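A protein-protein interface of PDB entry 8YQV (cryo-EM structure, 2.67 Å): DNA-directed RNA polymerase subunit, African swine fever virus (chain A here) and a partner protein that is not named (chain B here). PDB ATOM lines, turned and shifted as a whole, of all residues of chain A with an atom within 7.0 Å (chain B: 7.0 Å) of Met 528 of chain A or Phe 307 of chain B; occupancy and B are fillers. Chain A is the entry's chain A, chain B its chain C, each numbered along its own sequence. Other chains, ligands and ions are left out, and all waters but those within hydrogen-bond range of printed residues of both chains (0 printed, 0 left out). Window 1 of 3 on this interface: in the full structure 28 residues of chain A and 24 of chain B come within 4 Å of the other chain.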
ATOM      1  N   MET A 522      24.929  -6.027  -1.706  1.00  0.00           N
ATOM      2  CA  MET A 522      24.258  -4.823  -1.246  1.00  0.00           C
ATOM      3  C   MET A 522      23.336  -4.332  -2.350  1.00  0.00           C
ATOM      4  O   MET A 522      23.582  -4.580  -3.529  1.00  0.00           O
ATOM      5  CB  MET A 522      25.261  -3.729  -0.871  1.00  0.00           C
ATOM      6  CG  MET A 522      26.380  -3.560  -1.866  1.00  0.00           C
ATOM      7  SD  MET A 522      27.857  -2.840  -1.145  1.00  0.00           S
ATOM      8  CE  MET A 522      28.925  -4.271  -1.120  1.00  0.00           C
ATOM      9  N   ASN A 523      22.275  -3.631  -1.965  1.00  0.00           N
ATOM     10  CA  ASN A 523      21.356  -3.090  -2.954  1.00  0.00           C
ATOM     11  C   ASN A 523      21.964  -1.855  -3.614  1.00  0.00           C
ATOM     12  O   ASN A 523      23.070  -1.425  -3.291  1.00  0.00           O
ATOM     13  CB  ASN A 523      19.998  -2.787  -2.323  1.00  0.00           C
ATOM     14  CG  ASN A 523      20.075  -1.789  -1.191  1.00  0.00           C
ATOM     15  OD1 ASN A 523      21.128  -1.237  -0.896  1.00  0.00           O
ATOM     16  ND2 ASN A 523      18.945  -1.547  -0.551  1.00  0.00           N
ATOM     17  N   LYS A 524      21.226  -1.273  -4.560  1.00  0.00           N
ATOM     18  CA  LYS A 524      21.750  -0.152  -5.331  1.00  0.00           C
ATOM     19  C   LYS A 524      22.077   1.040  -4.441  1.00  0.00           C
ATOM     20  O   LYS A 524      23.095   1.708  -4.637  1.00  0.00           O
ATOM     21  CB  LYS A 524      20.748   0.249  -6.409  1.00  0.00           C
ATOM     22  CG  LYS A 524      21.138   1.472  -7.197  1.00  0.00           C
ATOM     23  CD  LYS A 524      20.032   1.876  -8.131  1.00  0.00           C
ATOM     24  CE  LYS A 524      20.361   3.140  -8.870  1.00  0.00           C
ATOM     25  NZ  LYS A 524      19.332   3.426  -9.885  1.00  0.00           N
ATOM     26  N   LEU A 525      21.219   1.328  -3.465  1.00  0.00           N
ATOM     27  CA  LEU A 525      21.425   2.479  -2.597  1.00  0.00           C
ATOM     28  C   LEU A 525      22.710   2.352  -1.790  1.00  0.00           C
ATOM     29  O   LEU A 525      23.441   3.331  -1.620  1.00  0.00           O
ATOM     30  CB  LEU A 525      20.229   2.640  -1.667  1.00  0.00           C
ATOM     31  CG  LEU A 525      20.274   3.765  -0.641  1.00  0.00           C
ATOM     32  CD1 LEU A 525      20.199   5.119  -1.311  1.00  0.00           C
ATOM     33  CD2 LEU A 525      19.145   3.588   0.331  1.00  0.00           C
ATOM     34  N   HIS A 526      22.987   1.163  -1.264  1.00  0.00           N
ATOM     35  CA  HIS A 526      24.186   0.967  -0.466  1.00  0.00           C
ATOM     36  C   HIS A 526      25.430   0.807  -1.322  1.00  0.00           C
ATOM     37  O   HIS A 526      26.527   1.133  -0.868  1.00  0.00           O
ATOM     38  CB  HIS A 526      24.001  -0.234   0.452  1.00  0.00           C
ATOM     39  CG  HIS A 526      23.026   0.012   1.556  1.00  0.00           C
ATOM     40  ND1 HIS A 526      21.664   0.026   1.356  1.00  0.00           N
ATOM     41  CD2 HIS A 526      23.215   0.268   2.869  1.00  0.00           C
ATOM     42  CE1 HIS A 526      21.056   0.277   2.499  1.00  0.00           C
ATOM     43  NE2 HIS A 526      21.974   0.422   3.434  1.00  0.00           N
ATOM     44  N   ALA A 527      25.291   0.298  -2.545  1.00  0.00           N
ATOM     45  CA  ALA A 527      26.415   0.297  -3.471  1.00  0.00           C
ATOM     46  C   ALA A 527      26.802   1.717  -3.850  1.00  0.00           C
ATOM     47  O   ALA A 527      27.988   2.050  -3.912  1.00  0.00           O
ATOM     48  CB  ALA A 527      26.070  -0.516  -4.713  1.00  0.00           C
ATOM     49  N   MET A 528      25.808   2.567  -4.102  1.00  0.00           N
ATOM     50  CA  MET A 528      26.057   3.978  -4.369  1.00  0.00           C
ATOM     51  C   MET A 528      26.718   4.659  -3.181  1.00  0.00           C
ATOM     52  O   MET A 528      27.594   5.507  -3.358  1.00  0.00           O
ATOM     53  CB  MET A 528      24.744   4.669  -4.726  1.00  0.00           C
ATOM     54  CG  MET A 528      24.498   4.810  -6.206  1.00  0.00           C
ATOM     55  SD  MET A 528      22.815   5.221  -6.682  1.00  0.00           S
ATOM     56  CE  MET A 528      22.151   5.788  -5.140  1.00  0.00           C
ATOM     57  N   GLY A 529      26.312   4.304  -1.964  1.00  0.00           N
ATOM     58  CA  GLY A 529      26.831   4.954  -0.777  1.00  0.00           C
ATOM     59  C   GLY A 529      28.282   4.658  -0.486  1.00  0.00           C
ATOM     60  O   GLY A 529      28.898   5.365   0.315  1.00  0.00           O
ATOM     61  N   LEU A 530      28.840   3.619  -1.095  1.00  0.00           N
ATOM     62  CA  LEU A 530      30.256   3.341  -0.912  1.00  0.00           C
ATOM     63  C   LEU A 530      31.116   4.347  -1.657  1.00  0.00           C
ATOM     64  O   LEU A 530      32.265   4.581  -1.275  1.00  0.00           O
ATOM     65  CB  LEU A 530      30.570   1.923  -1.375  1.00  0.00           C
ATOM     66  CG  LEU A 530      30.699   0.838  -0.313  1.00  0.00           C
ATOM     67  CD1 LEU A 530      29.431   0.710   0.467  1.00  0.00           C
ATOM     68  CD2 LEU A 530      31.028  -0.468  -0.967  1.00  0.00           C
ATOM     69  N   PHE A 531      30.574   4.956  -2.706  1.00  0.00           N
ATOM     70  CA  PHE A 531      31.304   5.868  -3.572  1.00  0.00           C
ATOM     71  C   PHE A 531      31.088   7.330  -3.231  1.00  0.00           C
ATOM     72  O   PHE A 531      31.747   8.189  -3.818  1.00  0.00           O
ATOM     73  CB  PHE A 531      30.902   5.636  -5.026  1.00  0.00           C
ATOM     74  CG  PHE A 531      31.492   4.406  -5.623  1.00  0.00           C
ATOM     75  CD1 PHE A 531      32.783   4.410  -6.101  1.00  0.00           C
ATOM     76  CD2 PHE A 531      30.759   3.245  -5.700  1.00  0.00           C
ATOM     77  CE1 PHE A 531      33.326   3.282  -6.650  1.00  0.00           C
ATOM     78  CE2 PHE A 531      31.298   2.120  -6.244  1.00  0.00           C
ATOM     79  CZ  PHE A 531      32.583   2.134  -6.717  1.00  0.00           C
ATOM     80  N   GLN A 532      30.191   7.641  -2.309  1.00  0.00           N
ATOM     81  CA  GLN A 532      29.820   9.024  -2.063  1.00  0.00           C
ATOM     82  C   GLN A 532      30.867   9.781  -1.274  1.00  0.00           C
ATOM     83  O   GLN A 532      30.611  10.908  -0.850  1.00  0.00           O
ATOM     84  CB  GLN A 532      28.468   9.088  -1.354  1.00  0.00           C
ATOM     85  CG  GLN A 532      28.465   8.584   0.057  1.00  0.00           C
ATOM     86  CD  GLN A 532      27.074   8.502   0.620  1.00  0.00           C
ATOM     87  OE1 GLN A 532      26.101   8.761  -0.074  1.00  0.00           O
ATOM     88  NE2 GLN A 532      26.969   8.141   1.884  1.00  0.00           N
ATOM     89  N   THR A 533      32.043   9.195  -1.095  1.00  0.00           N
ATOM     90  CA  THR A 533      33.102   9.781  -0.299  1.00  0.00           C
ATOM     91  C   THR A 533      34.464   9.700  -0.982  1.00  0.00           C
ATOM     92  O   THR A 533      35.361  10.470  -0.628  1.00  0.00           O
ATOM     93  CB  THR A 533      33.122   9.102   1.085  1.00  0.00           C
ATOM     94  OG1 THR A 533      32.120   9.696   1.916  1.00  0.00           O
ATOM     95  CG2 THR A 533      34.430   9.230   1.780  1.00  0.00           C
ATOM     96  N   PRO A 538      31.668   9.723  -9.702  1.00  0.00           N
ATOM     97  CA  PRO A 538      30.800   8.612  -9.339  1.00  0.00           C
ATOM     98  C   PRO A 538      30.524   7.726 -10.539  1.00  0.00           C
ATOM     99  O   PRO A 538      30.383   8.218 -11.671  1.00  0.00           O
ATOM    100  CB  PRO A 538      29.518   9.311  -8.856  1.00  0.00           C
ATOM    101  CG  PRO A 538      29.924  10.700  -8.567  1.00  0.00           C
ATOM    102  CD  PRO A 538      30.998  11.018  -9.532  1.00  0.00           C
ATOM    103  N   PRO A 539      30.445   6.416 -10.344  1.00  0.00           N
ATOM    104  CA  PRO A 539      30.056   5.530 -11.444  1.00  0.00           C
ATOM    105  C   PRO A 539      28.598   5.735 -11.818  1.00  0.00           C
ATOM    106  O   PRO A 539      27.864   6.511 -11.207  1.00  0.00           O
ATOM    107  CB  PRO A 539      30.299   4.131 -10.878  1.00  0.00           C
ATOM    108  CG  PRO A 539      31.217   4.335  -9.736  1.00  0.00           C
ATOM    109  CD  PRO A 539      30.853   5.656  -9.158  1.00  0.00           C
ATOM    110  N   CYS A 540      28.183   5.032 -12.860  1.00  0.00           N
ATOM    111  CA  CYS A 540      26.805   5.076 -13.320  1.00  0.00           C
ATOM    112  C   CYS A 540      26.083   3.847 -12.794  1.00  0.00           C
ATOM    113  O   CYS A 540      26.502   2.714 -13.052  1.00  0.00           O
ATOM    114  CB  CYS A 540      26.733   5.140 -14.842  1.00  0.00           C
ATOM    115  SG  CYS A 540      25.089   5.461 -15.498  1.00  0.00           S
ATOM    116  N   PHE A 541      25.013   4.072 -12.038  1.00  0.00           N
ATOM    117  CA  PHE A 541      24.176   3.003 -11.522  1.00  0.00           C
ATOM    118  C   PHE A 541      22.817   2.975 -12.204  1.00  0.00           C
ATOM    119  O   PHE A 541      21.867   2.419 -11.655  1.00  0.00           O
ATOM    120  CB  PHE A 541      24.005   3.145 -10.010  1.00  0.00           C
ATOM    121  CG  PHE A 541      25.260   2.897  -9.227  1.00  0.00           C
ATOM    122  CD1 PHE A 541      26.193   3.899  -9.053  1.00  0.00           C
ATOM    123  CD2 PHE A 541      25.493   1.674  -8.642  1.00  0.00           C
ATOM    124  CE1 PHE A 541      27.333   3.679  -8.326  1.00  0.00           C
ATOM    125  CE2 PHE A 541      26.632   1.453  -7.917  1.00  0.00           C
ATOM    126  CZ  PHE A 541      27.551   2.458  -7.760  1.00  0.00           C
ATOM    127  N   ALA A 542      22.703   3.571 -13.390  1.00  0.00           N
ATOM    128  CA  ALA A 542      21.406   3.700 -14.039  1.00  0.00           C
ATOM    129  C   ALA A 542      20.811   2.361 -14.434  1.00  0.00           C
ATOM    130  O   ALA A 542      19.584   2.235 -14.481  1.00  0.00           O
ATOM    131  CB  ALA A 542      21.517   4.593 -15.269  1.00  0.00           C
ATOM    132  N   LEU A 550      24.303  -6.043  -5.639  1.00  0.00           N
ATOM    133  CA  LEU A 550      25.633  -5.926  -6.216  1.00  0.00           C
ATOM    134  C   LEU A 550      26.638  -6.623  -5.316  1.00  0.00           C
ATOM    135  O   LEU A 550      26.660  -6.386  -4.108  1.00  0.00           O
ATOM    136  CB  LEU A 550      26.026  -4.463  -6.397  1.00  0.00           C
ATOM    137  CG  LEU A 550      25.385  -3.691  -7.545  1.00  0.00           C
ATOM    138  CD1 LEU A 550      24.077  -3.067  -7.120  1.00  0.00           C
ATOM    139  CD2 LEU A 550      26.345  -2.645  -8.044  1.00  0.00           C
ATOM    140  N   VAL A 555      31.428  -3.862  -7.020  1.00  0.00           N
ATOM    141  CA  VAL A 555      31.628  -2.478  -6.614  1.00  0.00           C
ATOM    142  C   VAL A 555      33.097  -2.090  -6.693  1.00  0.00           C
ATOM    143  O   VAL A 555      33.426  -0.972  -7.095  1.00  0.00           O
ATOM    144  CB  VAL A 555      31.044  -2.275  -5.206  1.00  0.00           C
ATOM    145  CG1 VAL A 555      31.437  -0.939  -4.643  1.00  0.00           C
ATOM    146  CG2 VAL A 555      29.542  -2.394  -5.259  1.00  0.00           C
ATOM    147  N   LYS B 295      18.910  12.567   0.202  1.00  0.00           N
ATOM    148  CA  LYS B 295      19.322  11.419  -0.595  1.00  0.00           C
ATOM    149  C   LYS B 295      18.218  10.375  -0.672  1.00  0.00           C
ATOM    150  O   LYS B 295      17.910   9.871  -1.757  1.00  0.00           O
ATOM    151  CB  LYS B 295      20.602  10.812  -0.026  1.00  0.00           C
ATOM    152  CG  LYS B 295      21.008   9.520  -0.698  1.00  0.00           C
ATOM    153  CD  LYS B 295      22.358   9.046  -0.230  1.00  0.00           C
ATOM    154  CE  LYS B 295      22.348   8.693   1.235  1.00  0.00           C
ATOM    155  NZ  LYS B 295      21.391   7.610   1.540  1.00  0.00           N
ATOM    156  N   ILE B 298      15.149  11.694  -2.813  1.00  0.00           N
ATOM    157  CA  ILE B 298      15.545  11.782  -4.213  1.00  0.00           C
ATOM    158  C   ILE B 298      15.614  10.395  -4.827  1.00  0.00           C
ATOM    159  O   ILE B 298      15.157  10.170  -5.952  1.00  0.00           O
ATOM    160  CB  ILE B 298      16.890  12.519  -4.341  1.00  0.00           C
ATOM    161  CG1 ILE B 298      16.719  14.009  -4.074  1.00  0.00           C
ATOM    162  CG2 ILE B 298      17.480  12.306  -5.709  1.00  0.00           C
ATOM    163  CD1 ILE B 298      18.016  14.717  -3.801  1.00  0.00           C
ATOM    164  N   TYR B 299      16.186   9.441  -4.093  1.00  0.00           N
ATOM    165  CA  TYR B 299      16.267   8.068  -4.565  1.00  0.00           C
ATOM    166  C   TYR B 299      14.891   7.438  -4.724  1.00  0.00           C
ATOM    167  O   TYR B 299      14.661   6.702  -5.685  1.00  0.00           O
ATOM    168  CB  TYR B 299      17.133   7.275  -3.595  1.00  0.00           C
ATOM    169  CG  TYR B 299      17.363   5.829  -3.933  1.00  0.00           C
ATOM    170  CD1 TYR B 299      18.077   5.462  -5.058  1.00  0.00           C
ATOM    171  CD2 TYR B 299      16.907   4.833  -3.097  1.00  0.00           C
ATOM    172  CE1 TYR B 299      18.301   4.146  -5.350  1.00  0.00           C
ATOM    173  CE2 TYR B 299      17.129   3.517  -3.382  1.00  0.00           C
ATOM    174  CZ  TYR B 299      17.825   3.179  -4.506  1.00  0.00           C
ATOM    175  OH  TYR B 299      18.049   1.861  -4.780  1.00  0.00           O
ATOM    176  N   PRO B 303      13.991   6.038  -8.975  1.00  0.00           N
ATOM    177  CA  PRO B 303      14.617   4.731  -8.735  1.00  0.00           C
ATOM    178  C   PRO B 303      15.765   4.415  -9.677  1.00  0.00           C
ATOM    179  O   PRO B 303      16.692   3.700  -9.280  1.00  0.00           O
ATOM    180  CB  PRO B 303      13.451   3.752  -8.920  1.00  0.00           C
ATOM    181  CG  PRO B 303      12.237   4.568  -8.718  1.00  0.00           C
ATOM    182  CD  PRO B 303      12.560   5.907  -9.275  1.00  0.00           C
ATOM    183  N   ASP B 304      15.734   4.913 -10.910  1.00  0.00           N
ATOM    184  CA  ASP B 304      16.772   4.642 -11.903  1.00  0.00           C
ATOM    185  C   ASP B 304      17.761   5.792 -12.024  1.00  0.00           C
ATOM    186  O   ASP B 304      18.244   6.099 -13.113  1.00  0.00           O
ATOM    187  CB  ASP B 304      16.142   4.338 -13.256  1.00  0.00           C
ATOM    188  CG  ASP B 304      15.176   5.409 -13.700  1.00  0.00           C
ATOM    189  OD1 ASP B 304      14.799   6.255 -12.868  1.00  0.00           O
ATOM    190  OD2 ASP B 304      14.799   5.411 -14.888  1.00  0.00           O
ATOM    191  N   ILE B 305      18.067   6.452 -10.910  1.00  0.00           N
ATOM    192  CA  ILE B 305      19.010   7.557 -10.927  1.00  0.00           C
ATOM    193  C   ILE B 305      20.425   7.024 -11.120  1.00  0.00           C
ATOM    194  O   ILE B 305      20.806   5.982 -10.572  1.00  0.00           O
ATOM    195  CB  ILE B 305      18.876   8.378  -9.630  1.00  0.00           C
ATOM    196  CG1 ILE B 305      19.694   9.660  -9.707  1.00  0.00           C
ATOM    197  CG2 ILE B 305      19.250   7.557  -8.415  1.00  0.00           C
ATOM    198  CD1 ILE B 305      19.318  10.656  -8.661  1.00  0.00           C
ATOM    199  N   SER B 306      21.206   7.726 -11.942  1.00  0.00           N
ATOM    200  CA  SER B 306      22.591   7.331 -12.170  1.00  0.00           C
ATOM    201  C   SER B 306      23.429   7.463 -10.908  1.00  0.00           C
ATOM    202  O   SER B 306      24.233   6.579 -10.606  1.00  0.00           O
ATOM    203  CB  SER B 306      23.196   8.157 -13.295  1.00  0.00           C
ATOM    204  OG  SER B 306      22.398   8.055 -14.454  1.00  0.00           O
ATOM    205  N   PHE B 307      23.261   8.548 -10.159  1.00  0.00           N
ATOM    206  CA  PHE B 307      23.939   8.662  -8.878  1.00  0.00           C
ATOM    207  C   PHE B 307      23.203   9.659  -8.005  1.00  0.00           C
ATOM    208  O   PHE B 307      22.744  10.692  -8.481  1.00  0.00           O
ATOM    209  CB  PHE B 307      25.394   9.100  -9.041  1.00  0.00           C
ATOM    210  CG  PHE B 307      26.205   8.991  -7.788  1.00  0.00           C
ATOM    211  CD1 PHE B 307      26.633   7.762  -7.333  1.00  0.00           C
ATOM    212  CD2 PHE B 307      26.544  10.118  -7.067  1.00  0.00           C
ATOM    213  CE1 PHE B 307      27.379   7.659  -6.186  1.00  0.00           C
ATOM    214  CE2 PHE B 307      27.290  10.017  -5.919  1.00  0.00           C
ATOM    215  CZ  PHE B 307      27.705   8.785  -5.478  1.00  0.00           C
ATOM    216  N   VAL B 308      23.077   9.327  -6.727  1.00  0.00           N
ATOM    217  CA  VAL B 308      22.752  10.315  -5.705  1.00  0.00           C
ATOM    218  C   VAL B 308      23.601  10.001  -4.486  1.00  0.00           C
ATOM    219  O   VAL B 308      23.709   8.844  -4.071  1.00  0.00           O
ATOM    220  CB  VAL B 308      21.247  10.361  -5.362  1.00  0.00           C
ATOM    221  CG1 VAL B 308      20.752   9.040  -4.837  1.00  0.00           C
ATOM    222  CG2 VAL B 308      20.967  11.474  -4.377  1.00  0.00           C
ATOM    223  N   GLY B 309      24.242  11.023  -3.941  1.00  0.00           N
ATOM    224  CA  GLY B 309      25.110  10.815  -2.799  1.00  0.00           C
ATOM    225  C   GLY B 309      25.283  12.118  -2.066  1.00  0.00           C
ATOM    226  O   GLY B 309      24.943  13.185  -2.572  1.00  0.00           O
ATOM    227  N   TYR B 310      25.806  12.024  -0.851  1.00  0.00           N
ATOM    228  CA  TYR B 310      26.048  13.212  -0.052  1.00  0.00           C
ATOM    229  C   TYR B 310      27.245  12.965   0.846  1.00  0.00           C
ATOM    230  O   TYR B 310      27.634  11.826   1.107  1.00  0.00           O
ATOM    231  CB  TYR B 310      24.819  13.608   0.772  1.00  0.00           C
ATOM    232  CG  TYR B 310      24.710  12.909   2.097  1.00  0.00           C
ATOM    233  CD1 TYR B 310      24.136  11.659   2.194  1.00  0.00           C
ATOM    234  CD2 TYR B 310      25.167  13.508   3.258  1.00  0.00           C
ATOM    235  CE1 TYR B 310      24.038  11.021   3.394  1.00  0.00           C
ATOM    236  CE2 TYR B 310      25.072  12.874   4.459  1.00  0.00           C
ATOM    237  CZ  TYR B 310      24.507  11.631   4.523  1.00  0.00           C
ATOM    238  OH  TYR B 310      24.406  10.990   5.730  1.00  0.00           O
ATOM    239  N   THR B 322      25.463  15.428  -4.254  1.00  0.00           N
ATOM    240  CA  THR B 322      25.722  15.266  -5.675  1.00  0.00           C
ATOM    241  C   THR B 322      24.648  14.383  -6.293  1.00  0.00           C
ATOM    242  O   THR B 322      24.337  13.313  -5.763  1.00  0.00           O
ATOM    243  CB  THR B 322      27.102  14.652  -5.904  1.00  0.00           C
ATOM    244  OG1 THR B 322      28.090  15.437  -5.230  1.00  0.00           O
ATOM    245  CG2 THR B 322      27.429  14.615  -7.376  1.00  0.00           C
ATOM    246  N   ILE B 323      24.085  14.835  -7.406  1.00  0.00           N
ATOM    247  CA  ILE B 323      23.069  14.105  -8.148  1.00  0.00           C
ATOM    248  C   ILE B 323      23.511  14.046  -9.601  1.00  0.00           C
ATOM    249  O   ILE B 323      23.943  15.056 -10.157  1.00  0.00           O
ATOM    250  CB  ILE B 323      21.690  14.780  -8.029  1.00  0.00           C
ATOM    251  CG1 ILE B 323      21.302  14.926  -6.565  1.00  0.00           C
ATOM    252  CG2 ILE B 323      20.644  13.991  -8.760  1.00  0.00           C
ATOM    253  CD1 ILE B 323      20.354  16.048  -6.306  1.00  0.00           C
ATOM    254  N   ILE B 324      23.433  12.869 -10.205  1.00  0.00           N
ATOM    255  CA  ILE B 324      23.751  12.678 -11.613  1.00  0.00           C
ATOM    256  C   ILE B 324      22.595  11.917 -12.232  1.00  0.00           C
ATOM    257  O   ILE B 324      22.266  10.816 -11.777  1.00  0.00           O
ATOM    258  CB  ILE B 324      25.069  11.918 -11.811  1.00  0.00           C
ATOM    259  CG1 ILE B 324      26.228  12.701 -11.210  1.00  0.00           C
ATOM    260  CG2 ILE B 324      25.314  11.685 -13.266  1.00  0.00           C
ATOM    261  CD1 ILE B 324      27.470  11.902 -11.047  1.00  0.00           C
ATOM    262  N   HIS B 325      21.981  12.495 -13.259  1.00  0.00           N
ATOM    263  CA  HIS B 325      20.753  11.930 -13.793  1.00  0.00           C
ATOM    264  C   HIS B 325      20.702  12.155 -15.294  1.00  0.00           C
ATOM    265  O   HIS B 325      21.394  13.013 -15.838  1.00  0.00           O
ATOM    266  CB  HIS B 325      19.528  12.530 -13.098  1.00  0.00           C
ATOM    267  CG  HIS B 325      18.237  11.875 -13.469  1.00  0.00           C
ATOM    268  ND1 HIS B 325      18.084  10.507 -13.507  1.00  0.00           N
ATOM    269  CD2 HIS B 325      17.027  12.397 -13.774  1.00  0.00           C
ATOM    270  CE1 HIS B 325      16.843  10.214 -13.848  1.00  0.00           C
ATOM    271  NE2 HIS B 325      16.180  11.343 -14.011  1.00  0.00           N
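NZ of Lys 524 of chain A sits close to O of Phe 541 of chain A, at 3.3 Å. The backbone NH of Ala 542 of chain A sits close to the side-chain sulfur of Cys 540 of chain A. The backbone NH (N) of Ser 306 of chain B lies close to the backbone carbonyl oxygen (O) of Ile 324 of chain B, at 3.3 Å. The backbone carbonyl oxygen of Phe 307 of chain B lies within hydrogen-bond range of the backbone NH of Ile 324 of chain B. The backbone carbonyl oxygen of Gly 309 of chain B lies within hydrogen-bond range of the backbone NH of Thr 322 of chain B.
Met 528 of chain A touches two residues of chain B. Of chain A, only Met 528 and Pro 538 come within 4 Å of Phe 307 of chain B. Printed residues of chain B within 4 Å of Lys 524 of chain A: Tyr 299 (3.5 Å), Pro 303 (2.7 Å), Asp 304 (3.5 Å) and Ile 305 (3.0 Å). Printed residues of chain A within 4 Å of Tyr 299 of chain B: Lys 524 and Leu 525. Printed residues of chain A within 4 Å of Tyr 310 of chain B: Gln 532. Of the printed residues of chain B, Ala 542 of chain A touches Ser 306 (3.7 Å). Phe 531 of chain A touches none of the printed residues of chain B. The nearest residue of chain A that does not touch Phe 307 of chain B is Gln 532 of chain A (4.02 Å). The nearest printed residue of chain B that does not touch Phe 541 of chain A is Phe 307 of chain B (4.3 Å).
Printed residues of chain A that touch a printed residue of chain B: Lys 524, Leu 525, Met 528, Gln 532, Pro 538, Pro 539, Cys 540, Phe 541 and Ala 542. Hydrophobic or aromatic side chains of chain A within 4 Å of the printed part of chain B: Leu 525, Met 528, Pro 538, Phe 541 and Ala 542. Hydrophobic or aromatic side chains of chain B that line the printed part of chain A: Tyr 299, Phe 307, Val 308 and Ile 324.
The backbone carbonyl oxygen of Pro 303 of chain B sits at hydrogen-bond distance from the side-chain amino group of Lys 524 of chain A (2.7 Å). NZ of Lys 524 of chain A is in hydrogen-bond range of O of Ile 305 of chain B, at 3.0 Å. The backbone NH of Leu 525 of chain A is in hydrogen-bond range of the side-chain hydroxyl of Tyr 299 of chain B, at 3.5 Å. The side-chain amide oxygen of Gln 532 of chain A lies within hydrogen-bond range of the backbone NH of Tyr 310 of chain B, at 3.4 Å. O of Ser 306 of chain B is in hydrogen-bond range of N of Phe 541 of chain A (3.0 Å).
Among the printed residues, merely in contact across the chains: Lys 524 of chain A with Tyr 299 of chain B (3.5 Å), Lys 524 of chain A with Asp 304 of chain B (3.5 Å), Leu 525 of chain A with Lys 295 of chain B (3.97 Å), Met 528 of chain A with Phe 307 of chain B (3.6 Å), Met 528 of chain A with Val 308 of chain B (3.6 Å), Gln 532 of chain A with Lys 295 of chain B (3.8 Å), Gln 532 of chain A with Gly 309 of chain B (3.6 Å), Pro 538 of chain A with Phe 307 of chain B (3.5 Å), Pro 538 of chain A with Ile 324 of chain B (3.7 Å), Pro 539 of chain A with Ser 306 of chain B (3.7 Å), Cys 540 of chain A with Ser 306 of chain B (3.9 Å), Phe 541 of chain A with Ile 305 of chain B (3.9 Å) and Ala 542 of chain A with Ser 306 of chain B (3.7 Å).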
